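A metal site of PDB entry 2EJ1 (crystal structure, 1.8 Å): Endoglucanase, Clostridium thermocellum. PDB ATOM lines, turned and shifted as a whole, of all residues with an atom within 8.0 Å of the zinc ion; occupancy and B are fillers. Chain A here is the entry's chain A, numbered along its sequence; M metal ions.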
ATOM      1  N   GLU A  33     -26.503   0.922  25.559  1.00  0.00           N
ATOM      2  CA  GLU A  33     -26.582   0.126  24.341  1.00  0.00           C
ATOM      3  C   GLU A  33     -25.327  -0.743  24.272  1.00  0.00           C
ATOM      4  O   GLU A  33     -24.234  -0.249  24.001  1.00  0.00           O
ATOM      5  CB  GLU A  33     -26.660   1.028  23.107  1.00  0.00           C
ATOM      6  CG  GLU A  33     -28.081   1.263  22.584  1.00  0.00           C
ATOM      7  CD  GLU A  33     -28.651   0.040  21.874  1.00  0.00           C
ATOM      8  OE1 GLU A  33     -27.959  -0.997  21.814  1.00  0.00           O
ATOM      9  OE2 GLU A  33     -29.794   0.115  21.382  1.00  0.00           O
ATOM     10  N   LEU A  34     -25.494  -2.031  24.532  1.00  0.00           N
ATOM     11  CA  LEU A  34     -24.377  -2.965  24.537  1.00  0.00           C
ATOM     12  C   LEU A  34     -24.245  -3.857  23.316  1.00  0.00           C
ATOM     13  O   LEU A  34     -25.183  -4.013  22.526  1.00  0.00           O
ATOM     14  CB  LEU A  34     -24.467  -3.870  25.763  1.00  0.00           C
ATOM     15  CG  LEU A  34     -24.589  -3.266  27.150  1.00  0.00           C
ATOM     16  CD1 LEU A  34     -24.778  -4.395  28.178  1.00  0.00           C
ATOM     17  CD2 LEU A  34     -23.354  -2.460  27.470  1.00  0.00           C
ATOM     18  N   ASP A  35     -23.057  -4.453  23.187  1.00  0.00           N
ATOM     19  CA  ASP A  35     -22.762  -5.398  22.114  1.00  0.00           C
ATOM     20  C   ASP A  35     -23.126  -6.746  22.738  1.00  0.00           C
ATOM     21  O   ASP A  35     -22.258  -7.592  22.977  1.00  0.00           O
ATOM     22  CB  ASP A  35     -21.271  -5.385  21.770  1.00  0.00           C
ATOM     23  CG  ASP A  35     -20.785  -4.015  21.302  1.00  0.00           C
ATOM     24  OD1 ASP A  35     -21.451  -3.437  20.420  1.00  0.00           O
ATOM     25  OD2 ASP A  35     -19.753  -3.536  21.807  1.00  0.00           O
ATOM     26  N   ALA A  36     -24.403  -6.903  23.035  1.00  0.00           N
ATOM     27  CA  ALA A  36     -24.886  -8.134  23.653  1.00  0.00           C
ATOM     28  C   ALA A  36     -26.392  -8.203  23.528  1.00  0.00           C
ATOM     29  O   ALA A  36     -27.061  -7.184  23.338  1.00  0.00           O
ATOM     30  CB  ALA A  36     -24.487  -8.169  25.128  1.00  0.00           C
ATOM     31  N   GLY A 365     -14.512  -4.870  33.280  1.00  0.00           N
ATOM     32  CA  GLY A 365     -15.309  -5.110  32.088  1.00  0.00           C
ATOM     33  C   GLY A 365     -14.588  -5.593  30.847  1.00  0.00           C
ATOM     34  O   GLY A 365     -15.188  -6.267  29.997  1.00  0.00           O
ATOM     35  N   ASP A 394     -20.788   0.885  29.574  1.00  0.00           N
ATOM     36  CA  ASP A 394     -20.880   0.943  28.112  1.00  0.00           C
ATOM     37  C   ASP A 394     -20.377  -0.273  27.331  1.00  0.00           C
ATOM     38  O   ASP A 394     -19.916  -1.259  27.898  1.00  0.00           O
ATOM     39  CB  ASP A 394     -20.191   2.210  27.590  1.00  0.00           C
ATOM     40  CG  ASP A 394     -18.702   2.224  27.849  1.00  0.00           C
ATOM     41  OD1 ASP A 394     -18.071   1.156  27.733  1.00  0.00           O
ATOM     42  OD2 ASP A 394     -18.162   3.301  28.165  1.00  0.00           O
ATOM     43  N   ALA A 395     -20.479  -0.175  26.007  1.00  0.00           N
ATOM     44  CA  ALA A 395     -20.086  -1.263  25.102  1.00  0.00           C
ATOM     45  C   ALA A 395     -18.599  -1.624  25.098  1.00  0.00           C
ATOM     46  O   ALA A 395     -18.203  -2.587  24.424  1.00  0.00           O
ATOM     47  CB  ALA A 395     -20.543  -0.938  23.681  1.00  0.00           C
ATOM     48  N   SER A 396     -17.775  -0.875  25.824  1.00  0.00           N
ATOM     49  CA  SER A 396     -16.344  -1.168  25.858  1.00  0.00           C
ATOM     50  C   SER A 396     -16.038  -2.321  26.813  1.00  0.00           C
ATOM     51  O   SER A 396     -14.927  -2.827  26.835  1.00  0.00           O
ATOM     52  CB  SER A 396     -15.554   0.073  26.283  1.00  0.00           C
ATOM     53  OG  SER A 396     -15.645   0.299  27.685  1.00  0.00           O
ATOM     54  N   ASN A 397     -17.022  -2.725  27.605  1.00  0.00           N
ATOM     55  CA  ASN A 397     -16.857  -3.823  28.546  1.00  0.00           C
ATOM     56  C   ASN A 397     -17.142  -5.137  27.824  1.00  0.00           C
ATOM     57  O   ASN A 397     -18.142  -5.790  28.090  1.00  0.00           O
ATOM     58  CB  ASN A 397     -17.812  -3.642  29.722  1.00  0.00           C
ATOM     59  CG  ASN A 397     -17.522  -2.397  30.528  1.00  0.00           C
ATOM     60  OD1 ASN A 397     -16.475  -2.294  31.166  1.00  0.00           O
ATOM     61  ND2 ASN A 397     -18.433  -1.429  30.485  1.00  0.00           N
ATOM     62  N   ASN A 398     -16.238  -5.515  26.914  1.00  0.00           N
ATOM     63  CA  ASN A 398     -16.428  -6.724  26.113  1.00  0.00           C
ATOM     64  C   ASN A 398     -16.609  -8.022  26.883  1.00  0.00           C
ATOM     65  O   ASN A 398     -17.376  -8.885  26.443  1.00  0.00           O
ATOM     66  CB  ASN A 398     -15.279  -6.865  25.092  1.00  0.00           C
ATOM     67  CG  ASN A 398     -13.901  -6.866  25.735  1.00  0.00           C
ATOM     68  OD1 ASN A 398     -13.545  -5.955  26.485  1.00  0.00           O
ATOM     69  ND2 ASN A 398     -13.107  -7.898  25.443  1.00  0.00           N
ATOM     70  N   TYR A 399     -15.903  -8.180  27.999  1.00  0.00           N
ATOM     71  CA  TYR A 399     -16.063  -9.415  28.777  1.00  0.00           C
ATOM     72  C   TYR A 399     -17.365  -9.391  29.569  1.00  0.00           C
ATOM     73  O   TYR A 399     -17.976 -10.437  29.786  1.00  0.00           O
ATOM     74  CB  TYR A 399     -14.846  -9.630  29.701  1.00  0.00           C
ATOM     75  CG  TYR A 399     -13.751 -10.407  29.014  1.00  0.00           C
ATOM     76  CD1 TYR A 399     -13.868 -11.778  28.797  1.00  0.00           C
ATOM     77  CD2 TYR A 399     -12.598  -9.766  28.555  1.00  0.00           C
ATOM     78  CE1 TYR A 399     -12.882 -12.497  28.126  1.00  0.00           C
ATOM     79  CE2 TYR A 399     -11.597 -10.476  27.887  1.00  0.00           C
ATOM     80  CZ  TYR A 399     -11.741 -11.838  27.678  1.00  0.00           C
ATOM     81  OH  TYR A 399     -10.755 -12.540  27.025  1.00  0.00           O
ATOM     82  N   THR A 400     -17.790  -8.212  30.016  1.00  0.00           N
ATOM     83  CA  THR A 400     -19.068  -8.126  30.725  1.00  0.00           C
ATOM     84  C   THR A 400     -20.139  -8.569  29.724  1.00  0.00           C
ATOM     85  O   THR A 400     -21.043  -9.328  30.047  1.00  0.00           O
ATOM     86  CB  THR A 400     -19.388  -6.684  31.179  1.00  0.00           C
ATOM     87  OG1 THR A 400     -18.316  -6.187  31.997  1.00  0.00           O
ATOM     88  CG2 THR A 400     -20.680  -6.669  32.013  1.00  0.00           C
ATOM     89  N   GLU A 401     -20.003  -8.083  28.496  1.00  0.00           N
ATOM     90  CA  GLU A 401     -20.955  -8.439  27.444  1.00  0.00           C
ATOM     91  C   GLU A 401     -20.925  -9.938  27.158  1.00  0.00           C
ATOM     92  O   GLU A 401     -21.971 -10.534  26.891  1.00  0.00           O
ATOM     93  CB  GLU A 401     -20.657  -7.639  26.185  1.00  0.00           C
ATOM     94  CG  GLU A 401     -20.836  -6.134  26.408  1.00  0.00           C
ATOM     95  CD  GLU A 401     -20.341  -5.294  25.247  1.00  0.00           C
ATOM     96  OE1 GLU A 401     -19.290  -5.655  24.674  1.00  0.00           O
ATOM     97  OE2 GLU A 401     -20.983  -4.269  24.933  1.00  0.00           O
ATOM     98  N   ALA A 402     -19.744 -10.533  27.210  1.00  0.00           N
ATOM     99  CA  ALA A 402     -19.640 -11.976  26.967  1.00  0.00           C
ATOM    100  C   ALA A 402     -20.379 -12.709  28.086  1.00  0.00           C
ATOM    101  O   ALA A 402     -21.049 -13.723  27.850  1.00  0.00           O
ATOM    102  CB  ALA A 402     -18.168 -12.396  26.941  1.00  0.00           C
ATOM    103  N   SER A 484     -12.976 -12.736  24.227  1.00  0.00           N
ATOM    104  CA  SER A 484     -14.268 -12.512  24.859  1.00  0.00           C
ATOM    105  C   SER A 484     -15.368 -13.054  23.931  1.00  0.00           C
ATOM    106  O   SER A 484     -16.532 -13.107  24.308  1.00  0.00           O
ATOM    107  CB  SER A 484     -14.484 -11.027  25.158  1.00  0.00           C
ATOM    108  OG  SER A 484     -14.255 -10.216  24.014  1.00  0.00           O
HETATM  109 ZN    ZN M   1     -18.762  -4.201  23.406  1.00  0.00          ZN
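Three residues have an atom within 4 Å of the zinc ion: Asp 35, Ala 395 and Glu 401. Along chain A the residues within 4 Å of the zinc ion span positions 35 to 401. The nearest printed residue that does not touch the zinc ion is Ser 396 (4.2 Å).
The zinc ion is bound by O of Ala 395 (2.0 Å), OD2 of Asp 35 (2.0 Å) and OE1 of Glu 401 (2.0 Å). The zinc ion has three donor atoms within binding distance. Slightly farther from the zinc ion lies OE2 of Glu 401 (2.7 Å).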
